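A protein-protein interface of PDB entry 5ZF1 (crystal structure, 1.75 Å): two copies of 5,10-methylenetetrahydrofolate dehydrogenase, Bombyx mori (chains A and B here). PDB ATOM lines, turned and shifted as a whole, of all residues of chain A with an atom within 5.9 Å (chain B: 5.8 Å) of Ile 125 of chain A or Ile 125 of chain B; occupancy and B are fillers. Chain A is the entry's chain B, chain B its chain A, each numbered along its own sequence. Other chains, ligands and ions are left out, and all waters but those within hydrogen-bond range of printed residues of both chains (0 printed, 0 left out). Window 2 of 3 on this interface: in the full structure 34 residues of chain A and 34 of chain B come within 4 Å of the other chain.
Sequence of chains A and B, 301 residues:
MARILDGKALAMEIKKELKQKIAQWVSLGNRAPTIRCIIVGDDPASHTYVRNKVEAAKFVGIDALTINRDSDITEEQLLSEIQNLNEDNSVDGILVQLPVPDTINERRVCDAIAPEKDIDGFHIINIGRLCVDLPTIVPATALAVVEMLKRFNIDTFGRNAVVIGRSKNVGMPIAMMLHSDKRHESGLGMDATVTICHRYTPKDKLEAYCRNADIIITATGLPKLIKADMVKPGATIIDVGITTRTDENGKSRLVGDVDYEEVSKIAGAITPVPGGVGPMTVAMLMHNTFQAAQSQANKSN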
ATOM      1  N   ASP A 111      35.637 -26.146  -0.303  1.00  0.00           N
ATOM      2  CA  ASP A 111      34.342 -26.779  -0.504  1.00  0.00           C
ATOM      3  C   ASP A 111      34.403 -28.300  -0.460  1.00  0.00           C
ATOM      4  O   ASP A 111      33.348 -28.945  -0.450  1.00  0.00           O
ATOM      5  CB  ASP A 111      33.727 -26.300  -1.826  1.00  0.00           C
ATOM      6  CG  ASP A 111      33.422 -24.810  -1.817  1.00  0.00           C
ATOM      7  OD1 ASP A 111      33.241 -24.255  -0.715  1.00  0.00           O
ATOM      8  OD2 ASP A 111      33.336 -24.181  -2.901  1.00  0.00           O
ATOM      9  N   PRO A 115      30.910 -29.674   5.466  1.00  0.00           N
ATOM     10  CA  PRO A 115      30.518 -28.467   6.216  1.00  0.00           C
ATOM     11  C   PRO A 115      30.429 -28.691   7.708  1.00  0.00           C
ATOM     12  O   PRO A 115      30.777 -27.797   8.488  1.00  0.00           O
ATOM     13  CB  PRO A 115      29.147 -28.115   5.618  1.00  0.00           C
ATOM     14  CG  PRO A 115      29.194 -28.672   4.231  1.00  0.00           C
ATOM     15  CD  PRO A 115      30.021 -29.929   4.313  1.00  0.00           C
ATOM     16  N   HIS A 123      33.552 -23.108   3.868  1.00  0.00           N
ATOM     17  CA  HIS A 123      32.710 -23.805   2.900  1.00  0.00           C
ATOM     18  C   HIS A 123      31.523 -22.926   2.511  1.00  0.00           C
ATOM     19  O   HIS A 123      30.939 -22.244   3.358  1.00  0.00           O
ATOM     20  CB  HIS A 123      32.223 -25.127   3.508  1.00  0.00           C
ATOM     21  CG  HIS A 123      31.603 -26.070   2.523  1.00  0.00           C
ATOM     22  ND1 HIS A 123      30.379 -25.836   1.933  1.00  0.00           N
ATOM     23  CD2 HIS A 123      32.020 -27.273   2.058  1.00  0.00           C
ATOM     24  CE1 HIS A 123      30.086 -26.836   1.121  1.00  0.00           C
ATOM     25  NE2 HIS A 123      31.066 -27.721   1.179  1.00  0.00           N
ATOM     26  N   ILE A 124      31.151 -22.956   1.223  1.00  0.00           N
ATOM     27  CA  ILE A 124      30.089 -22.063   0.758  1.00  0.00           C
ATOM     28  C   ILE A 124      28.795 -22.271   1.534  1.00  0.00           C
ATOM     29  O   ILE A 124      28.047 -21.311   1.768  1.00  0.00           O
ATOM     30  CB  ILE A 124      29.873 -22.207  -0.767  1.00  0.00           C
ATOM     31  CG1 ILE A 124      29.623 -23.658  -1.149  1.00  0.00           C
ATOM     32  CG2 ILE A 124      31.052 -21.605  -1.515  1.00  0.00           C
ATOM     33  CD1 ILE A 124      29.087 -23.829  -2.561  1.00  0.00           C
ATOM     34  N   ILE A 125      28.511 -23.507   1.968  1.00  0.00           N
ATOM     35  CA  ILE A 125      27.308 -23.746   2.762  1.00  0.00           C
ATOM     36  C   ILE A 125      27.399 -23.021   4.097  1.00  0.00           C
ATOM     37  O   ILE A 125      26.415 -22.448   4.575  1.00  0.00           O
ATOM     38  CB  ILE A 125      27.068 -25.256   2.947  1.00  0.00           C
ATOM     39  CG1 ILE A 125      26.604 -25.875   1.618  1.00  0.00           C
ATOM     40  CG2 ILE A 125      26.043 -25.514   4.041  1.00  0.00           C
ATOM     41  CD1 ILE A 125      26.540 -27.407   1.622  1.00  0.00           C
ATOM     42  N   ASN A 126      28.575 -23.025   4.721  1.00  0.00           N
ATOM     43  CA  ASN A 126      28.693 -22.321   5.996  1.00  0.00           C
ATOM     44  C   ASN A 126      28.656 -20.812   5.803  1.00  0.00           C
ATOM     45  O   ASN A 126      28.056 -20.089   6.610  1.00  0.00           O
ATOM     46  CB  ASN A 126      29.971 -22.740   6.728  1.00  0.00           C
ATOM     47  CG  ASN A 126      29.877 -24.152   7.305  1.00  0.00           C
ATOM     48  OD1 ASN A 126      28.808 -24.584   7.729  1.00  0.00           O
ATOM     49  ND2 ASN A 126      31.004 -24.868   7.335  1.00  0.00           N
ATOM     50  N   ILE A 127      29.294 -20.317   4.744  1.00  0.00           N
ATOM     51  CA  ILE A 127      29.242 -18.890   4.451  1.00  0.00           C
ATOM     52  C   ILE A 127      27.822 -18.485   4.102  1.00  0.00           C
ATOM     53  O   ILE A 127      27.333 -17.429   4.527  1.00  0.00           O
ATOM     54  CB  ILE A 127      30.221 -18.549   3.313  1.00  0.00           C
ATOM     55  CG1 ILE A 127      31.670 -18.727   3.784  1.00  0.00           C
ATOM     56  CG2 ILE A 127      29.978 -17.115   2.789  1.00  0.00           C
ATOM     57  CD1 ILE A 127      32.149 -17.636   4.722  1.00  0.00           C
ATOM     58  N   GLY A 128      27.132 -19.324   3.324  1.00  0.00           N
ATOM     59  CA  GLY A 128      25.748 -19.031   2.992  1.00  0.00           C
ATOM     60  C   GLY A 128      24.872 -18.884   4.222  1.00  0.00           C
ATOM     61  O   GLY A 128      24.079 -17.947   4.321  1.00  0.00           O
ATOM     62  N   ARG A 129      25.024 -19.790   5.188  1.00  0.00           N
ATOM     63  CA  ARG A 129      24.225 -19.698   6.404  1.00  0.00           C
ATOM     64  C   ARG A 129      24.579 -18.450   7.206  1.00  0.00           C
ATOM     65  O   ARG A 129      23.695 -17.803   7.786  1.00  0.00           O
ATOM     66  CB  ARG A 129      24.397 -20.974   7.235  1.00  0.00           C
ATOM     67  CG  ARG A 129      23.778 -22.223   6.576  1.00  0.00           C
ATOM     68  CD  ARG A 129      23.888 -23.464   7.457  1.00  0.00           C
ATOM     69  NE  ARG A 129      23.181 -23.297   8.724  1.00  0.00           N
ATOM     70  CZ  ARG A 129      21.882 -23.521   8.903  1.00  0.00           C
ATOM     71  NH1 ARG A 129      21.124 -23.938   7.893  1.00  0.00           N
ATOM     72  NH2 ARG A 129      21.342 -23.332  10.098  1.00  0.00           N
ATOM     73  N   LEU A 130      25.864 -18.079   7.244  1.00  0.00           N
ATOM     74  CA  LEU A 130      26.240 -16.835   7.903  1.00  0.00           C
ATOM     75  C   LEU A 130      25.505 -15.657   7.280  1.00  0.00           C
ATOM     76  O   LEU A 130      24.993 -14.782   7.989  1.00  0.00           O
ATOM     77  CB  LEU A 130      27.748 -16.605   7.802  1.00  0.00           C
ATOM     78  CG  LEU A 130      28.260 -15.287   8.388  1.00  0.00           C
ATOM     79  CD1 LEU A 130      28.046 -15.300   9.880  1.00  0.00           C
ATOM     80  CD2 LEU A 130      29.716 -15.041   8.064  1.00  0.00           C
ATOM     81  N   THR A 136      25.613 -21.238  12.154  1.00  0.00           N
ATOM     82  CA  THR A 136      26.565 -21.876  11.249  1.00  0.00           C
ATOM     83  C   THR A 136      27.907 -22.009  11.966  1.00  0.00           C
ATOM     84  O   THR A 136      28.024 -21.717  13.161  1.00  0.00           O
ATOM     85  CB  THR A 136      26.656 -21.070   9.939  1.00  0.00           C
ATOM     86  OG1 THR A 136      27.391 -21.800   8.954  1.00  0.00           O
ATOM     87  CG2 THR A 136      27.353 -19.733  10.148  1.00  0.00           C
ATOM     88  N   ASP B 111      15.911 -24.857   0.756  1.00  0.00           N
ATOM     89  CA  ASP B 111      16.986 -25.806   0.544  1.00  0.00           C
ATOM     90  C   ASP B 111      16.498 -27.126  -0.029  1.00  0.00           C
ATOM     91  O   ASP B 111      17.328 -27.957  -0.413  1.00  0.00           O
ATOM     92  CB  ASP B 111      17.750 -26.027   1.854  1.00  0.00           C
ATOM     93  CG  ASP B 111      18.611 -24.825   2.230  1.00  0.00           C
ATOM     94  OD1 ASP B 111      18.913 -24.007   1.323  1.00  0.00           O
ATOM     95  OD2 ASP B 111      18.989 -24.707   3.421  1.00  0.00           O
ATOM     96  N   PRO B 115      19.518 -27.041  -6.213  1.00  0.00           N
ATOM     97  CA  PRO B 115      20.188 -25.768  -6.551  1.00  0.00           C
ATOM     98  C   PRO B 115      20.232 -25.485  -8.035  1.00  0.00           C
ATOM     99  O   PRO B 115      20.170 -24.320  -8.441  1.00  0.00           O
ATOM    100  CB  PRO B 115      21.602 -25.951  -5.977  1.00  0.00           C
ATOM    101  CG  PRO B 115      21.446 -26.981  -4.893  1.00  0.00           C
ATOM    102  CD  PRO B 115      20.351 -27.908  -5.360  1.00  0.00           C
ATOM    103  N   HIS B 123      18.389 -20.995  -2.551  1.00  0.00           N
ATOM    104  CA  HIS B 123      19.057 -22.138  -1.929  1.00  0.00           C
ATOM    105  C   HIS B 123      20.366 -21.677  -1.298  1.00  0.00           C
ATOM    106  O   HIS B 123      21.077 -20.835  -1.850  1.00  0.00           O
ATOM    107  CB  HIS B 123      19.339 -23.233  -2.953  1.00  0.00           C
ATOM    108  CG  HIS B 123      19.753 -24.537  -2.344  1.00  0.00           C
ATOM    109  ND1 HIS B 123      21.051 -24.805  -1.962  1.00  0.00           N
ATOM    110  CD2 HIS B 123      19.042 -25.657  -2.073  1.00  0.00           C
ATOM    111  CE1 HIS B 123      21.117 -26.028  -1.465  1.00  0.00           C
ATOM    112  NE2 HIS B 123      19.909 -26.565  -1.517  1.00  0.00           N
ATOM    113  N   ILE B 124      20.680 -22.231  -0.125  1.00  0.00           N
ATOM    114  CA  ILE B 124      21.859 -21.777   0.608  1.00  0.00           C
ATOM    115  C   ILE B 124      23.136 -21.933  -0.215  1.00  0.00           C
ATOM    116  O   ILE B 124      24.076 -21.136  -0.070  1.00  0.00           O
ATOM    117  CB  ILE B 124      21.936 -22.512   1.968  1.00  0.00           C
ATOM    118  CG1 ILE B 124      22.803 -21.709   2.934  1.00  0.00           C
ATOM    119  CG2 ILE B 124      22.420 -23.936   1.801  1.00  0.00           C
ATOM    120  CD1 ILE B 124      22.122 -20.472   3.385  1.00  0.00           C
ATOM    121  N   ILE B 125      23.193 -22.931  -1.106  1.00  0.00           N
ATOM    122  CA  ILE B 125      24.365 -23.107  -1.954  1.00  0.00           C
ATOM    123  C   ILE B 125      24.474 -21.965  -2.951  1.00  0.00           C
ATOM    124  O   ILE B 125      25.560 -21.424  -3.182  1.00  0.00           O
ATOM    125  CB  ILE B 125      24.303 -24.474  -2.660  1.00  0.00           C
ATOM    126  CG1 ILE B 125      24.570 -25.599  -1.641  1.00  0.00           C
ATOM    127  CG2 ILE B 125      25.234 -24.521  -3.864  1.00  0.00           C
ATOM    128  CD1 ILE B 125      24.470 -27.000  -2.228  1.00  0.00           C
ATOM    129  N   ASN B 126      23.352 -21.570  -3.547  1.00  0.00           N
ATOM    130  CA  ASN B 126      23.376 -20.449  -4.480  1.00  0.00           C
ATOM    131  C   ASN B 126      23.708 -19.136  -3.769  1.00  0.00           C
ATOM    132  O   ASN B 126      24.485 -18.320  -4.289  1.00  0.00           O
ATOM    133  CB  ASN B 126      22.036 -20.382  -5.224  1.00  0.00           C
ATOM    134  CG  ASN B 126      21.913 -21.486  -6.272  1.00  0.00           C
ATOM    135  OD1 ASN B 126      22.882 -21.816  -6.935  1.00  0.00           O
ATOM    136  ND2 ASN B 126      20.725 -22.060  -6.417  1.00  0.00           N
ATOM    137  N   ILE B 127      23.182 -18.945  -2.554  1.00  0.00           N
ATOM    138  CA  ILE B 127      23.492 -17.744  -1.784  1.00  0.00           C
ATOM    139  C   ILE B 127      24.968 -17.736  -1.394  1.00  0.00           C
ATOM    140  O   ILE B 127      25.649 -16.708  -1.508  1.00  0.00           O
ATOM    141  CB  ILE B 127      22.580 -17.648  -0.541  1.00  0.00           C
ATOM    142  CG1 ILE B 127      21.122 -17.346  -0.935  1.00  0.00           C
ATOM    143  CG2 ILE B 127      23.061 -16.552   0.413  1.00  0.00           C
ATOM    144  CD1 ILE B 127      20.915 -15.929  -1.420  1.00  0.00           C
ATOM    145  N   GLY B 128      25.485 -18.881  -0.935  1.00  0.00           N
ATOM    146  CA  GLY B 128      26.878 -18.940  -0.522  1.00  0.00           C
ATOM    147  C   GLY B 128      27.828 -18.609  -1.651  1.00  0.00           C
ATOM    148  O   GLY B 128      28.833 -17.921  -1.451  1.00  0.00           O
ATOM    149  N   ARG B 129      27.523 -19.096  -2.859  1.00  0.00           N
ATOM    150  CA  ARG B 129      28.352 -18.750  -4.011  1.00  0.00           C
ATOM    151  C   ARG B 129      28.281 -17.258  -4.311  1.00  0.00           C
ATOM    152  O   ARG B 129      29.300 -16.640  -4.637  1.00  0.00           O
ATOM    153  CB  ARG B 129      27.926 -19.566  -5.237  1.00  0.00           C
ATOM    154  CG  ARG B 129      28.244 -21.053  -5.129  1.00  0.00           C
ATOM    155  CD  ARG B 129      27.755 -21.832  -6.363  1.00  0.00           C
ATOM    156  NE  ARG B 129      28.367 -21.368  -7.608  1.00  0.00           N
ATOM    157  CZ  ARG B 129      29.517 -21.814  -8.107  1.00  0.00           C
ATOM    158  NH1 ARG B 129      30.203 -22.747  -7.458  1.00  0.00           N
ATOM    159  NH2 ARG B 129      29.989 -21.321  -9.257  1.00  0.00           N
ATOM    160  N   LEU B 130      27.087 -16.662  -4.207  1.00  0.00           N
ATOM    161  CA  LEU B 130      26.964 -15.221  -4.386  1.00  0.00           C
ATOM    162  C   LEU B 130      27.895 -14.483  -3.438  1.00  0.00           C
ATOM    163  O   LEU B 130      28.599 -13.541  -3.830  1.00  0.00           O
ATOM    164  CB  LEU B 130      25.521 -14.783  -4.135  1.00  0.00           C
ATOM    165  CG  LEU B 130      25.280 -13.283  -4.293  1.00  0.00           C
ATOM    166  CD1 LEU B 130      25.469 -12.812  -5.743  1.00  0.00           C
ATOM    167  CD2 LEU B 130      23.900 -12.922  -3.765  1.00  0.00           C
ATOM    168  N   THR B 136      26.653 -17.745 -10.007  1.00  0.00           N
ATOM    169  CA  THR B 136      25.591 -18.437  -9.294  1.00  0.00           C
ATOM    170  C   THR B 136      24.263 -18.048  -9.934  1.00  0.00           C
ATOM    171  O   THR B 136      24.221 -17.279 -10.900  1.00  0.00           O
ATOM    172  CB  THR B 136      25.649 -18.072  -7.804  1.00  0.00           C
ATOM    173  OG1 THR B 136      24.844 -18.979  -7.058  1.00  0.00           O
ATOM    174  CG2 THR B 136      25.121 -16.668  -7.583  1.00  0.00           C
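Hydrophobic or aromatic side chains of chain B within 4 Å of the printed part of chain A: Ile 124 and Ile 125.
Of the 11 printed residues of chain A, 4 touch a printed residue of chain B.
O of Ile 124 of chain A touches CA of Gly 128 of chain B, 3.5 Å away.
CG of Arg 129 of chain B touches CD1 of Ile 124 of chain A, 3.9 Å away.
Ile 125 of chain B touches Ile 125 of chain A.
Gly 128 of chain A touches Ile 124 of chain B (C to CD1, 3.3 Å).
CA of Gly 128 of chain A touches CA of Gly 128 of chain B, 3.7 Å away.
CD1 of Ile 124 of chain B touches N of Arg 129 of chain A (3.5 Å).
Ile 124 of chain A touches Gly 128 of chain B, and with the chains exchanged Gly 128 of chain A touches Ile 124 of chain B.
Ile 124 of chain A touches Arg 129 of chain B, and with the chains exchanged Arg 129 of chain A touches Ile 124 of chain B.
Ile 125 of chain B touches its own counterpart, Ile 125 of chain A.
Gly 128 of chain A touches its own counterpart, Gly 128 of chain B.
Positions printed for both chains: 111, 115, 123, 124, 125, 126, 127, 128, 129, 130 and 136.
Of the 6 pairs that touch across the chains among the printed residues, 6 have their exchanged pair printed and touching as well.
The side-chain carboxylate (OD1) of Asp 111 of chain B lies within hydrogen-bond range of the backbone NH (N) of Ile 124 of chain B (2.9 Å).
ND1 of His 123 of chain B lies within hydrogen-bond range of N of Ile 125 of chain B (3.0 Å).
N of Ile 124 of chain A lies within hydrogen-bond range of OD1 of Asp 111 of chain A (3.1 Å).
A ring nitrogen (ND1) of His 123 of chain A sits at hydrogen-bond distance from the backbone NH (N) of Ile 125 of chain A, 3.0 Å away.
Of the printed residues of chain B, Ile 124 of chain A touches Gly 128 and Arg 129.
Of chain B, only Ile 125 comes within 4 Å of Ile 125 of chain A.
Of the printed residues of chain B, Arg 129 of chain A touches Ile 124.
Ile 125 of chain B touches just one residue of chain A: Ile 125.
Printed residues of chain A within 4 Å of Arg 129 of chain B: Ile 124.
The nearest printed residue of chain B that does not touch Ile 124 of chain A is Ile 125 of chain B (4.1 Å).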
